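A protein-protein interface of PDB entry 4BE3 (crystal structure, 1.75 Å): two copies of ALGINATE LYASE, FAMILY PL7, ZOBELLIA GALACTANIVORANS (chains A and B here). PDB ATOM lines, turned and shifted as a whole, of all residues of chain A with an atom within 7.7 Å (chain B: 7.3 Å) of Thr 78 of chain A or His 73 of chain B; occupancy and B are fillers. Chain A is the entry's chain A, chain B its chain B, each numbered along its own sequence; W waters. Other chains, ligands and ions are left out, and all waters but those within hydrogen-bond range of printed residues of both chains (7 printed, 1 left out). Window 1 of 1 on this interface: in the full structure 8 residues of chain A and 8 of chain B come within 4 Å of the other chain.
O of Ile 75 of chain A lies within hydrogen-bond range of OG1 of Thr 78 of chain A. O of Ile 253 of chain B is in hydrogen-bond range of N of Asp 113 of chain B (2.8 Å). The backbone carbonyl oxygen of Ile 75 of chain B lies within hydrogen-bond range of the side-chain hydroxyl of Thr 78 of chain B. The backbone NH (N) of Gly 251 of chain A sits at hydrogen-bond distance from the side-chain carboxylate (OE1) of Glu 77 of chain A. The backbone carbonyl oxygen (O) of Lys 71 of chain B lies close to a ring nitrogen (NE2) of His 73 of chain B (3.4 Å).
Among the printed residues, pairs that only touch across the chains: Lys 72 of chain A with Gly 79 of chain B (3.7 Å), His 73 of chain A with Thr 78 of chain B (3.5 Å), Ile 75 of chain A with Ile 75 of chain B (3.7 Å), Glu 77 of chain A with Ile 253 of chain B (3.7 Å), Thr 78 of chain A with His 73 of chain B (3.4 Å), Thr 78 of chain A with Ile 253 of chain B (3.8 Å), Gly 79 of chain A with Lys 72 of chain B (3.7 Å) and Ser 307 of chain A with Lys 72 of chain B (3.6 Å).
Of the printed residues of chain B, Glu 77 of chain A touches Ile 253 (3.7 Å). Printed residues of chain B within 4 Å of Thr 78 of chain A: His 73 and Ile 253. Of the printed residues of chain B, Gly 79 of chain A touches Lys 72. Lys 81 of chain A touches none of the printed residues of chain B. Gly 306 of chain A touches none of the printed residues of chain B. Of the printed residues of chain A, Lys 72 of chain B touches Gly 79 (3.7 Å) and Ser 307 (3.6 Å).
Hydrophobic or aromatic side chains of chain A that line the printed part of chain B: Ile 75. Among the printed residues, no Asp or Glu carboxylate lies within 4 Å of a Lys or Arg side-chain nitrogen of the other chain.
Lys 72 of chain A touches Gly 79 of chain B, and with the chains exchanged Gly 79 of chain A touches Lys 72 of chain B. His 73 of chain A touches Thr 78 of chain B, and with the chains exchanged Thr 78 of chain A touches His 73 of chain B. Ile 75 of chain B touches its own counterpart, Ile 75 of chain A. 6 positions are printed for both chains. Of the 8 pairs that touch across the chains among the printed residues, 5 have their exchanged pair printed and touching as well.
Water W2 lies within hydrogen-bond range of the side-chain amino group of Lys 72 of chain A, the backbone carbonyl oxygen of Gly 79 of chain B and the side-chain hydroxyl of Thr 78 of chain B. Water W4 lies within hydrogen-bond range of the side-chain amino group of Lys 72 of chain B (2.5 Å) and the backbone carbonyl oxygen of Gly 79 of chain A (2.8 Å). Water W7 lies within hydrogen-bond range of the side-chain amino group of Lys 72 of chain B (2.6 Å), the backbone carbonyl oxygen of Gly 79 of chain A (2.7 Å) and the side-chain hydroxyl of Thr 78 of chain A (2.9 Å). Water W3 lies within hydrogen-bond range of O of Thr 78 of chain A (2.9 Å) and N of His 73 of chain B (2.9 Å). Water W6 lies within hydrogen-bond range of the backbone NH of His 73 of chain A and the backbone carbonyl oxygen of Thr 78 of chain B. Water W5 bridges the backbone carbonyl oxygen (O) of Lys 72 of chain A (3.1 Å) and the side-chain amino group (NZ) of Lys 72 of chain B (3.4 Å).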
ATOM      1  N   LYS A  72      25.881  -3.228 -22.405  1.00  0.00           N
ATOM      2  CA  LYS A  72      25.717  -2.791 -21.004  1.00  0.00           C
ATOM      3  C   LYS A  72      27.081  -2.471 -20.373  1.00  0.00           C
ATOM      4  O   LYS A  72      27.907  -3.372 -20.332  1.00  0.00           O
ATOM      5  CB  LYS A  72      25.091  -3.937 -20.236  1.00  0.00           C
ATOM      6  CG  LYS A  72      24.471  -3.377 -18.836  1.00  0.00           C
ATOM      7  CD  LYS A  72      23.545  -4.444 -18.248  1.00  0.00           C
ATOM      8  CE  LYS A  72      22.627  -3.877 -17.155  1.00  0.00           C
ATOM      9  NZ  LYS A  72      23.651  -3.729 -16.060  1.00  0.00           N
ATOM     10  N   HIS A  73      27.297  -1.250 -19.927  1.00  0.00           N
ATOM     11  CA  HIS A  73      28.629  -0.846 -19.519  1.00  0.00           C
ATOM     12  C   HIS A  73      28.790  -1.112 -18.029  1.00  0.00           C
ATOM     13  O   HIS A  73      27.753  -1.387 -17.327  1.00  0.00           O
ATOM     14  CB  HIS A  73      28.773   0.592 -19.844  1.00  0.00           C
ATOM     15  CG  HIS A  73      28.657   0.888 -21.300  1.00  0.00           C
ATOM     16  ND1 HIS A  73      28.559   2.183 -21.779  1.00  0.00           N
ATOM     17  CD2 HIS A  73      28.597   0.065 -22.396  1.00  0.00           C
ATOM     18  CE1 HIS A  73      28.486   2.158 -23.130  1.00  0.00           C
ATOM     19  NE2 HIS A  73      28.543   0.871 -23.516  1.00  0.00           N
ATOM     20  N   TRP A  74      29.976  -0.957 -17.459  1.00  0.00           N
ATOM     21  CA  TRP A  74      30.205  -1.228 -16.073  1.00  0.00           C
ATOM     22  C   TRP A  74      31.472  -0.536 -15.655  1.00  0.00           C
ATOM     23  O   TRP A  74      32.266  -0.152 -16.482  1.00  0.00           O
ATOM     24  CB  TRP A  74      30.280  -2.745 -15.781  1.00  0.00           C
ATOM     25  CG  TRP A  74      31.098  -3.454 -16.875  1.00  0.00           C
ATOM     26  CD1 TRP A  74      30.690  -3.896 -18.138  1.00  0.00           C
ATOM     27  CD2 TRP A  74      32.502  -3.808 -16.751  1.00  0.00           C
ATOM     28  NE1 TRP A  74      31.764  -4.531 -18.781  1.00  0.00           N
ATOM     29  CE2 TRP A  74      32.866  -4.497 -17.991  1.00  0.00           C
ATOM     30  CE3 TRP A  74      33.460  -3.673 -15.714  1.00  0.00           C
ATOM     31  CZ2 TRP A  74      34.149  -4.932 -18.255  1.00  0.00           C
ATOM     32  CZ3 TRP A  74      34.788  -4.137 -15.985  1.00  0.00           C
ATOM     33  CH2 TRP A  74      35.098  -4.774 -17.251  1.00  0.00           C
ATOM     34  N   ILE A  75      31.595  -0.240 -14.356  1.00  0.00           N
ATOM     35  CA  ILE A  75      32.851   0.286 -13.799  1.00  0.00           C
ATOM     36  C   ILE A  75      33.594  -0.902 -13.189  1.00  0.00           C
ATOM     37  O   ILE A  75      33.070  -1.982 -12.884  1.00  0.00           O
ATOM     38  CB  ILE A  75      32.582   1.407 -12.761  1.00  0.00           C
ATOM     39  CG1 ILE A  75      31.728   0.868 -11.526  1.00  0.00           C
ATOM     40  CG2 ILE A  75      31.844   2.551 -13.412  1.00  0.00           C
ATOM     41  CD1 ILE A  75      31.725   1.959 -10.387  1.00  0.00           C
ATOM     42  N   PRO A  76      34.952  -0.766 -13.082  1.00  0.00           N
ATOM     43  CA  PRO A  76      35.722  -1.931 -12.606  1.00  0.00           C
ATOM     44  C   PRO A  76      35.264  -2.432 -11.259  1.00  0.00           C
ATOM     45  O   PRO A  76      35.283  -3.638 -11.026  1.00  0.00           O
ATOM     46  CB  PRO A  76      37.179  -1.392 -12.543  1.00  0.00           C
ATOM     47  CG  PRO A  76      37.149  -0.368 -13.811  1.00  0.00           C
ATOM     48  CD  PRO A  76      35.803   0.408 -13.475  1.00  0.00           C
ATOM     49  N   GLU A  77      34.832  -1.516 -10.352  1.00  0.00           N
ATOM     50  CA  GLU A  77      34.382  -1.981  -9.077  1.00  0.00           C
ATOM     51  C   GLU A  77      33.235  -2.925  -9.161  1.00  0.00           C
ATOM     52  O   GLU A  77      33.073  -3.753  -8.220  1.00  0.00           O
ATOM     53  CB  GLU A  77      33.886  -0.740  -8.273  1.00  0.00           C
ATOM     54  CG  GLU A  77      35.067   0.177  -7.838  1.00  0.00           C
ATOM     55  CD  GLU A  77      35.398   1.289  -8.830  1.00  0.00           C
ATOM     56  OE1 GLU A  77      35.215   1.195 -10.076  1.00  0.00           O
ATOM     57  OE2 GLU A  77      35.924   2.346  -8.344  1.00  0.00           O
ATOM     58  N   THR A  78      32.336  -2.759 -10.150  1.00  0.00           N
ATOM     59  CA  THR A  78      31.213  -3.702 -10.153  1.00  0.00           C
ATOM     60  C   THR A  78      31.540  -4.890 -11.034  1.00  0.00           C
ATOM     61  O   THR A  78      30.912  -5.898 -10.917  1.00  0.00           O
ATOM     62  CB  THR A  78      29.869  -3.066 -10.670  1.00  0.00           C
ATOM     63  OG1 THR A  78      30.107  -2.557 -11.980  1.00  0.00           O
ATOM     64  CG2 THR A  78      29.627  -1.848  -9.744  1.00  0.00           C
ATOM     65  N   GLY A  79      32.441  -4.729 -11.979  1.00  0.00           N
ATOM     66  CA  GLY A  79      33.034  -6.015 -12.572  1.00  0.00           C
ATOM     67  C   GLY A  79      32.344  -6.569 -13.735  1.00  0.00           C
ATOM     68  O   GLY A  79      31.324  -6.011 -14.245  1.00  0.00           O
ATOM     69  N   GLY A  80      32.965  -7.651 -14.282  1.00  0.00           N
ATOM     70  CA  GLY A  80      32.389  -8.259 -15.450  1.00  0.00           C
ATOM     71  C   GLY A  80      33.383  -9.358 -15.888  1.00  0.00           C
ATOM     72  O   GLY A  80      34.571  -9.281 -15.512  1.00  0.00           O
ATOM     73  N   LYS A  81      32.899 -10.289 -16.642  1.00  0.00           N
ATOM     74  CA  LYS A  81      33.782 -11.416 -17.123  1.00  0.00           C
ATOM     75  C   LYS A  81      33.467 -11.691 -18.514  1.00  0.00           C
ATOM     76  O   LYS A  81      32.267 -11.757 -18.975  1.00  0.00           O
ATOM     77  CB  LYS A  81      33.479 -12.648 -16.245  1.00  0.00           C
ATOM     78  CG  LYS A  81      34.391 -13.823 -16.623  1.00  0.00           C
ATOM     79  CD  LYS A  81      33.969 -15.130 -15.900  1.00  0.00           C
ATOM     80  CE  LYS A  81      34.184 -14.976 -14.410  1.00  0.00           C
ATOM     81  NZ  LYS A  81      33.771 -16.265 -13.723  1.00  0.00           N
ATOM     82  N   VAL A 193      36.930  -9.377 -14.188  1.00  0.00           N
ATOM     83  CA  VAL A 193      37.197  -8.187 -13.353  1.00  0.00           C
ATOM     84  C   VAL A 193      36.254  -8.323 -12.156  1.00  0.00           C
ATOM     85  O   VAL A 193      35.044  -8.371 -12.365  1.00  0.00           O
ATOM     86  CB  VAL A 193      36.895  -6.858 -14.086  1.00  0.00           C
ATOM     87  CG1 VAL A 193      37.131  -5.677 -13.139  1.00  0.00           C
ATOM     88  CG2 VAL A 193      37.920  -6.776 -15.346  1.00  0.00           C
ATOM     89  N   TYR A 194      36.828  -8.489 -11.005  1.00  0.00           N
ATOM     90  CA  TYR A 194      36.048  -8.647  -9.752  1.00  0.00           C
ATOM     91  C   TYR A 194      36.496  -7.644  -8.736  1.00  0.00           C
ATOM     92  O   TYR A 194      37.689  -7.631  -8.341  1.00  0.00           O
ATOM     93  CB  TYR A 194      36.269 -10.090  -9.279  1.00  0.00           C
ATOM     94  CG  TYR A 194      35.462 -10.352  -8.022  1.00  0.00           C
ATOM     95  CD1 TYR A 194      34.079 -10.390  -8.102  1.00  0.00           C
ATOM     96  CD2 TYR A 194      36.103 -10.511  -6.804  1.00  0.00           C
ATOM     97  CE1 TYR A 194      33.324 -10.646  -6.918  1.00  0.00           C
ATOM     98  CE2 TYR A 194      35.365 -10.748  -5.615  1.00  0.00           C
ATOM     99  CZ  TYR A 194      34.008 -10.816  -5.723  1.00  0.00           C
ATOM    100  OH  TYR A 194      33.282 -11.052  -4.579  1.00  0.00           O
ATOM    101  N   GLU A 195      35.549  -6.763  -8.286  1.00  0.00           N
ATOM    102  CA  GLU A 195      35.863  -5.756  -7.363  1.00  0.00           C
ATOM    103  C   GLU A 195      37.093  -4.909  -7.790  1.00  0.00           C
ATOM    104  O   GLU A 195      37.944  -4.575  -6.979  1.00  0.00           O
ATOM    105  CB  GLU A 195      36.109  -6.387  -5.977  1.00  0.00           C
ATOM    106  CG  GLU A 195      34.764  -6.980  -5.556  1.00  0.00           C
ATOM    107  CD  GLU A 195      34.777  -7.460  -4.077  1.00  0.00           C
ATOM    108  OE1 GLU A 195      35.853  -7.666  -3.446  1.00  0.00           O
ATOM    109  OE2 GLU A 195      33.687  -7.686  -3.584  1.00  0.00           O
ATOM    110  N   GLY A 196      37.143  -4.602  -9.054  1.00  0.00           N
ATOM    111  CA  GLY A 196      38.129  -3.649  -9.519  1.00  0.00           C
ATOM    112  C   GLY A 196      39.476  -4.317  -9.867  1.00  0.00           C
ATOM    113  O   GLY A 196      40.396  -3.584 -10.256  1.00  0.00           O
ATOM    114  N   LEU A 217      42.138  -0.291  -9.933  1.00  0.00           N
ATOM    115  CA  LEU A 217      41.748   0.808  -9.050  1.00  0.00           C
ATOM    116  C   LEU A 217      42.913   1.563  -8.462  1.00  0.00           C
ATOM    117  O   LEU A 217      42.677   2.610  -7.855  1.00  0.00           O
ATOM    118  CB  LEU A 217      40.932   0.255  -7.842  1.00  0.00           C
ATOM    119  CG  LEU A 217      39.701  -0.639  -8.165  1.00  0.00           C
ATOM    120  CD1 LEU A 217      38.931  -1.012  -6.852  1.00  0.00           C
ATOM    121  CD2 LEU A 217      38.741   0.049  -9.131  1.00  0.00           C
ATOM    122  N   GLY A 251      36.032   3.761 -11.115  1.00  0.00           N
ATOM    123  CA  GLY A 251      34.842   4.537 -11.374  1.00  0.00           C
ATOM    124  C   GLY A 251      34.667   4.950 -12.824  1.00  0.00           C
ATOM    125  O   GLY A 251      33.764   5.701 -13.190  1.00  0.00           O
ATOM    126  N   GLY A 306      29.681 -12.616 -18.473  1.00  0.00           N
ATOM    127  CA  GLY A 306      29.026 -12.926 -17.126  1.00  0.00           C
ATOM    128  C   GLY A 306      29.554 -11.942 -16.087  1.00  0.00           C
ATOM    129  O   GLY A 306      30.150 -10.883 -16.400  1.00  0.00           O
ATOM    130  N   SER A 307      29.214 -12.249 -14.837  1.00  0.00           N
ATOM    131  CA  SER A 307      29.569 -11.336 -13.828  1.00  0.00           C
ATOM    132  C   SER A 307      31.036 -11.721 -13.408  1.00  0.00           C
ATOM    133  O   SER A 307      31.467 -12.844 -13.474  1.00  0.00           O
ATOM    134  CB  SER A 307      28.362 -11.326 -12.799  1.00  0.00           C
ATOM    135  OG  SER A 307      28.643 -12.462 -12.244  1.00  0.00           O
ATOM    136  N   GLY A 308      31.745 -10.700 -12.922  1.00  0.00           N
ATOM    137  CA  GLY A 308      33.034 -10.889 -12.274  1.00  0.00           C
ATOM    138  C   GLY A 308      32.900 -11.869 -11.079  1.00  0.00           C
ATOM    139  O   GLY A 308      31.812 -11.919 -10.389  1.00  0.00           O
ATOM    140  N   SER A 309      33.918 -12.663 -10.818  1.00  0.00           N
ATOM    141  CA  SER A 309      33.892 -13.592  -9.685  1.00  0.00           C
ATOM    142  C   SER A 309      35.177 -13.658  -8.941  1.00  0.00           C
ATOM    143  O   SER A 309      36.249 -13.508  -9.460  1.00  0.00           O
ATOM    144  CB  SER A 309      33.459 -14.995 -10.130  1.00  0.00           C
ATOM    145  OG  SER A 309      34.330 -15.568 -11.080  1.00  0.00           O
ATOM    146  N   LYS B  15      20.457 -12.979  -4.281  1.00  0.00           N
ATOM    147  CA  LYS B  15      20.721 -13.646  -3.032  1.00  0.00           C
ATOM    148  C   LYS B  15      19.484 -13.325  -2.135  1.00  0.00           C
ATOM    149  O   LYS B  15      18.688 -12.510  -2.556  1.00  0.00           O
ATOM    150  CB  LYS B  15      21.961 -13.139  -2.345  1.00  0.00           C
ATOM    151  CG  LYS B  15      21.897 -11.601  -1.947  1.00  0.00           C
ATOM    152  CD  LYS B  15      23.308 -11.135  -1.506  1.00  0.00           C
ATOM    153  CE  LYS B  15      24.119 -10.768  -2.705  1.00  0.00           C
ATOM    154  NZ  LYS B  15      25.346  -9.933  -2.396  1.00  0.00           N
ATOM    155  N   GLY B  69      18.258  -9.747  -2.928  1.00  0.00           N
ATOM    156  CA  GLY B  69      19.079  -8.614  -3.248  1.00  0.00           C
ATOM    157  C   GLY B  69      19.823  -9.016  -4.525  1.00  0.00           C
ATOM    158  O   GLY B  69      20.288 -10.169  -4.657  1.00  0.00           O
ATOM    159  N   GLN B  70      19.905  -8.129  -5.517  1.00  0.00           N
ATOM    160  CA  GLN B  70      20.536  -8.468  -6.810  1.00  0.00           C
ATOM    161  C   GLN B  70      22.067  -8.583  -6.558  1.00  0.00           C
ATOM    162  O   GLN B  70      22.701  -7.683  -5.984  1.00  0.00           O
ATOM    163  CB  GLN B  70      20.248  -7.286  -7.715  1.00  0.00           C
ATOM    164  CG  GLN B  70      20.956  -7.381  -9.073  1.00  0.00           C
ATOM    165  CD  GLN B  70      20.607  -6.222  -9.956  1.00  0.00           C
ATOM    166  OE1 GLN B  70      20.350  -5.093  -9.442  1.00  0.00           O
ATOM    167  NE2 GLN B  70      20.693  -6.442 -11.284  1.00  0.00           N
ATOM    168  N   LYS B  71      22.690  -9.658  -7.128  1.00  0.00           N
ATOM    169  CA  LYS B  71      24.125  -9.868  -6.827  1.00  0.00           C
ATOM    170  C   LYS B  71      25.015  -8.900  -7.628  1.00  0.00           C
ATOM    171  O   LYS B  71      26.070  -8.490  -7.130  1.00  0.00           O
ATOM    172  CB  LYS B  71      24.497 -11.279  -7.253  1.00  0.00           C
ATOM    173  CG  LYS B  71      23.796 -12.348  -6.334  1.00  0.00           C
ATOM    174  CD  LYS B  71      24.176 -13.772  -6.960  1.00  0.00           C
ATOM    175  CE  LYS B  71      23.630 -14.901  -6.077  1.00  0.00           C
ATOM    176  NZ  LYS B  71      23.950 -16.270  -6.764  1.00  0.00           N
ATOM    177  N   LYS B  72      24.596  -8.595  -8.832  1.00  0.00           N
ATOM    178  CA  LYS B  72      25.536  -7.769  -9.708  1.00  0.00           C
ATOM    179  C   LYS B  72      25.170  -6.280  -9.588  1.00  0.00           C
ATOM    180  O   LYS B  72      24.046  -5.929  -9.976  1.00  0.00           O
ATOM    181  CB  LYS B  72      25.391  -8.162 -11.199  1.00  0.00           C
ATOM    182  CG  LYS B  72      26.513  -7.498 -12.107  1.00  0.00           C
ATOM    183  CD  LYS B  72      26.532  -8.240 -13.425  1.00  0.00           C
ATOM    184  CE  LYS B  72      27.850  -7.999 -14.278  1.00  0.00           C
ATOM    185  NZ  LYS B  72      27.734  -6.586 -14.709  1.00  0.00           N
ATOM    186  N   HIS B  73      26.051  -5.470  -9.049  1.00  0.00           N
ATOM    187  CA  HIS B  73      25.658  -4.090  -8.742  1.00  0.00           C
ATOM    188  C   HIS B  73      25.923  -3.178  -9.881  1.00  0.00           C
ATOM    189  O   HIS B  73      26.562  -3.620 -10.879  1.00  0.00           O
ATOM    190  CB  HIS B  73      26.479  -3.663  -7.594  1.00  0.00           C
ATOM    191  CG  HIS B  73      26.322  -4.526  -6.374  1.00  0.00           C
ATOM    192  ND1 HIS B  73      27.215  -4.494  -5.339  1.00  0.00           N
ATOM    193  CD2 HIS B  73      25.434  -5.527  -6.085  1.00  0.00           C
ATOM    194  CE1 HIS B  73      26.792  -5.349  -4.375  1.00  0.00           C
ATOM    195  NE2 HIS B  73      25.742  -6.006  -4.853  1.00  0.00           N
ATOM    196  N   TRP B  74      25.502  -1.908  -9.784  1.00  0.00           N
ATOM    197  CA  TRP B  74      25.608  -0.995 -10.928  1.00  0.00           C
ATOM    198  C   TRP B  74      25.517   0.413 -10.428  1.00  0.00           C
ATOM    199  O   TRP B  74      24.965   0.624  -9.357  1.00  0.00           O
ATOM    200  CB  TRP B  74      24.504  -1.272 -11.984  1.00  0.00           C
ATOM    201  CG  TRP B  74      23.137  -1.567 -11.383  1.00  0.00           C
ATOM    202  CD1 TRP B  74      22.661  -2.778 -10.849  1.00  0.00           C
ATOM    203  CD2 TRP B  74      22.114  -0.594 -11.156  1.00  0.00           C
ATOM    204  NE1 TRP B  74      21.336  -2.592 -10.395  1.00  0.00           N
ATOM    205  CE2 TRP B  74      20.981  -1.307 -10.521  1.00  0.00           C
ATOM    206  CE3 TRP B  74      21.991   0.799 -11.400  1.00  0.00           C
ATOM    207  CZ2 TRP B  74      19.760  -0.659 -10.191  1.00  0.00           C
ATOM    208  CZ3 TRP B  74      20.732   1.432 -11.060  1.00  0.00           C
ATOM    209  CH2 TRP B  74      19.676   0.729 -10.420  1.00  0.00           C
ATOM    210  N   ILE B  75      26.042   1.374 -11.191  1.00  0.00           N
ATOM    211  CA  ILE B  75      25.836   2.751 -10.834  1.00  0.00           C
ATOM    212  C   ILE B  75      24.682   3.267 -11.715  1.00  0.00           C
ATOM    213  O   ILE B  75      24.354   2.717 -12.750  1.00  0.00           O
ATOM    214  CB  ILE B  75      27.158   3.577 -11.042  1.00  0.00           C
ATOM    215  CG1 ILE B  75      27.656   3.548 -12.550  1.00  0.00           C
ATOM    216  CG2 ILE B  75      28.249   3.085 -10.045  1.00  0.00           C
ATOM    217  CD1 ILE B  75      28.782   4.681 -12.713  1.00  0.00           C
ATOM    218  N   THR B  78      25.038   3.591 -15.516  1.00  0.00           N
ATOM    219  CA  THR B  78      25.034   2.473 -16.394  1.00  0.00           C
ATOM    220  C   THR B  78      23.650   1.786 -16.370  1.00  0.00           C
ATOM    221  O   THR B  78      23.301   1.044 -17.308  1.00  0.00           O
ATOM    222  CB  THR B  78      26.133   1.402 -16.057  1.00  0.00           C
ATOM    223  OG1 THR B  78      25.962   0.901 -14.744  1.00  0.00           O
ATOM    224  CG2 THR B  78      27.568   2.105 -16.155  1.00  0.00           C
ATOM    225  N   GLY B  79      22.972   1.882 -15.232  1.00  0.00           N
ATOM    226  CA  GLY B  79      21.537   1.589 -15.334  1.00  0.00           C
ATOM    227  C   GLY B  79      21.151   0.182 -15.033  1.00  0.00           C
ATOM    228  O   GLY B  79      22.015  -0.750 -14.686  1.00  0.00           O
ATOM    229  N   HIS B 111      18.892  -0.069  -3.622  1.00  0.00           N
ATOM    230  CA  HIS B 111      19.561   0.200  -2.351  1.00  0.00           C
ATOM    231  C   HIS B 111      21.033   0.440  -2.657  1.00  0.00           C
ATOM    232  O   HIS B 111      21.653  -0.286  -3.491  1.00  0.00           O
ATOM    233  CB  HIS B 111      19.355  -1.065  -1.497  1.00  0.00           C
ATOM    234  CG  HIS B 111      20.055  -0.956  -0.196  1.00  0.00           C
ATOM    235  ND1 HIS B 111      21.211  -1.542   0.076  1.00  0.00           N
ATOM    236  CD2 HIS B 111      19.648  -0.311   0.986  1.00  0.00           C
ATOM    237  CE1 HIS B 111      21.602  -1.230   1.389  1.00  0.00           C
ATOM    238  NE2 HIS B 111      20.658  -0.456   1.902  1.00  0.00           N
ATOM    239  N   ASP B 113      24.996   0.307  -2.151  1.00  0.00           N
ATOM    240  CA  ASP B 113      25.925  -0.574  -1.471  1.00  0.00           C
ATOM    241  C   ASP B 113      27.061   0.169  -0.734  1.00  0.00           C
ATOM    242  O   ASP B 113      27.916  -0.491  -0.122  1.00  0.00           O
ATOM    243  CB  ASP B 113      26.604  -1.476  -2.562  1.00  0.00           C
ATOM    244  CG  ASP B 113      27.282  -2.691  -1.905  1.00  0.00           C
ATOM    245  OD1 ASP B 113      26.764  -3.358  -0.991  1.00  0.00           O
ATOM    246  OD2 ASP B 113      28.406  -2.907  -2.341  1.00  0.00           O
ATOM    247  N   GLU B 252      27.366   6.193  -7.505  1.00  0.00           N
ATOM    248  CA  GLU B 252      27.308   5.419  -6.301  1.00  0.00           C
ATOM    249  C   GLU B 252      26.720   4.014  -6.651  1.00  0.00           C
ATOM    250  O   GLU B 252      25.646   3.893  -7.290  1.00  0.00           O
ATOM    251  CB  GLU B 252      26.401   6.166  -5.262  1.00  0.00           C
ATOM    252  CG  GLU B 252      26.576   5.457  -3.948  1.00  0.00           C
ATOM    253  CD  GLU B 252      26.124   6.350  -2.831  1.00  0.00           C
ATOM    254  OE1 GLU B 252      26.800   7.404  -2.547  1.00  0.00           O
ATOM    255  OE2 GLU B 252      25.020   5.986  -2.337  1.00  0.00           O
ATOM    256  N   ILE B 253      27.411   2.983  -6.206  1.00  0.00           N
ATOM    257  CA  ILE B 253      27.071   1.613  -6.584  1.00  0.00           C
ATOM    258  C   ILE B 253      25.729   1.217  -5.859  1.00  0.00           C
ATOM    259  O   ILE B 253      25.628   1.429  -4.642  1.00  0.00           O
ATOM    260  CB  ILE B 253      28.188   0.679  -6.196  1.00  0.00           C
ATOM    261  CG1 ILE B 253      29.388   1.036  -7.130  1.00  0.00           C
ATOM    262  CG2 ILE B 253      27.825  -0.805  -6.461  1.00  0.00           C
ATOM    263  CD1 ILE B 253      30.630   0.260  -6.705  1.00  0.00           C
ATOM    264  N   GLN B 254      24.800   0.659  -6.622  1.00  0.00           N
ATOM    265  CA  GLN B 254      23.386   0.356  -6.118  1.00  0.00           C
ATOM    266  C   GLN B 254      23.071  -1.031  -6.611  1.00  0.00           C
ATOM    267  O   GLN B 254      23.744  -1.631  -7.512  1.00  0.00           O
ATOM    268  CB  GLN B 254      22.350   1.197  -6.941  1.00  0.00           C
ATOM    269  CG  GLN B 254      22.440   2.732  -7.163  1.00  0.00           C
ATOM    270  CD  GLN B 254      22.490   3.383  -5.772  1.00  0.00           C
ATOM    271  OE1 GLN B 254      21.717   3.019  -4.865  1.00  0.00           O
ATOM    272  NE2 GLN B 254      23.360   4.366  -5.593  1.00  0.00           N
ATOM    273  N   TYR B 255      21.981  -1.596  -6.081  1.00  0.00           N
ATOM    274  CA  TYR B 255      21.446  -2.798  -6.690  1.00  0.00           C
ATOM    275  C   TYR B 255      19.936  -2.922  -6.320  1.00  0.00           C
ATOM    276  O   TYR B 255      19.492  -2.223  -5.395  1.00  0.00           O
ATOM    277  CB  TYR B 255      22.221  -4.038  -6.144  1.00  0.00           C
ATOM    278  CG  TYR B 255      22.250  -4.151  -4.660  1.00  0.00           C
ATOM    279  CD1 TYR B 255      21.271  -4.876  -3.983  1.00  0.00           C
ATOM    280  CD2 TYR B 255      23.341  -3.595  -3.917  1.00  0.00           C
ATOM    281  CE1 TYR B 255      21.303  -4.976  -2.566  1.00  0.00           C
ATOM    282  CE2 TYR B 255      23.400  -3.719  -2.490  1.00  0.00           C
ATOM    283  CZ  TYR B 255      22.381  -4.407  -1.866  1.00  0.00           C
ATOM    284  OH  TYR B 255      22.452  -4.602  -0.530  1.00  0.00           O
ATOM    285  N   PHE B 256      19.211  -3.712  -7.089  1.00  0.00           N
ATOM    286  CA  PHE B 256      17.778  -3.830  -6.847  1.00  0.00           C
ATOM    287  C   PHE B 256      17.524  -4.840  -5.748  1.00  0.00           C
ATOM    288  O   PHE B 256      18.316  -5.747  -5.474  1.00  0.00           O
ATOM    289  CB  PHE B 256      17.082  -4.445  -8.033  1.00  0.00           C
ATOM    290  CG  PHE B 256      16.959  -3.469  -9.187  1.00  0.00           C
ATOM    291  CD1 PHE B 256      16.166  -2.318  -9.058  1.00  0.00           C
ATOM    292  CD2 PHE B 256      17.536  -3.729 -10.446  1.00  0.00           C
ATOM    293  CE1 PHE B 256      16.025  -1.383 -10.124  1.00  0.00           C
ATOM    294  CE2 PHE B 256      17.353  -2.858 -11.547  1.00  0.00           C
ATOM    295  CZ  PHE B 256      16.626  -1.664 -11.377  1.00  0.00           C
HETATM  296  O   HOH W   1      21.931  -3.467 -14.064  1.00  0.00           O
HETATM  297  O   HOH W   2      24.534  -1.462 -15.576  1.00  0.00           O
HETATM  298  O   HOH W   3      28.851  -6.099  -8.936  1.00  0.00           O
HETATM  299  O   HOH W   4      29.589  -6.605 -16.380  1.00  0.00           O
HETATM  300  O   HOH W   5      27.570  -5.145 -17.800  1.00  0.00           O
HETATM  301  O   HOH W   6      25.183   0.710 -19.539  1.00  0.00           O
HETATM  302  O   HOH W   7      29.088  -4.927 -13.258  1.00  0.00           O
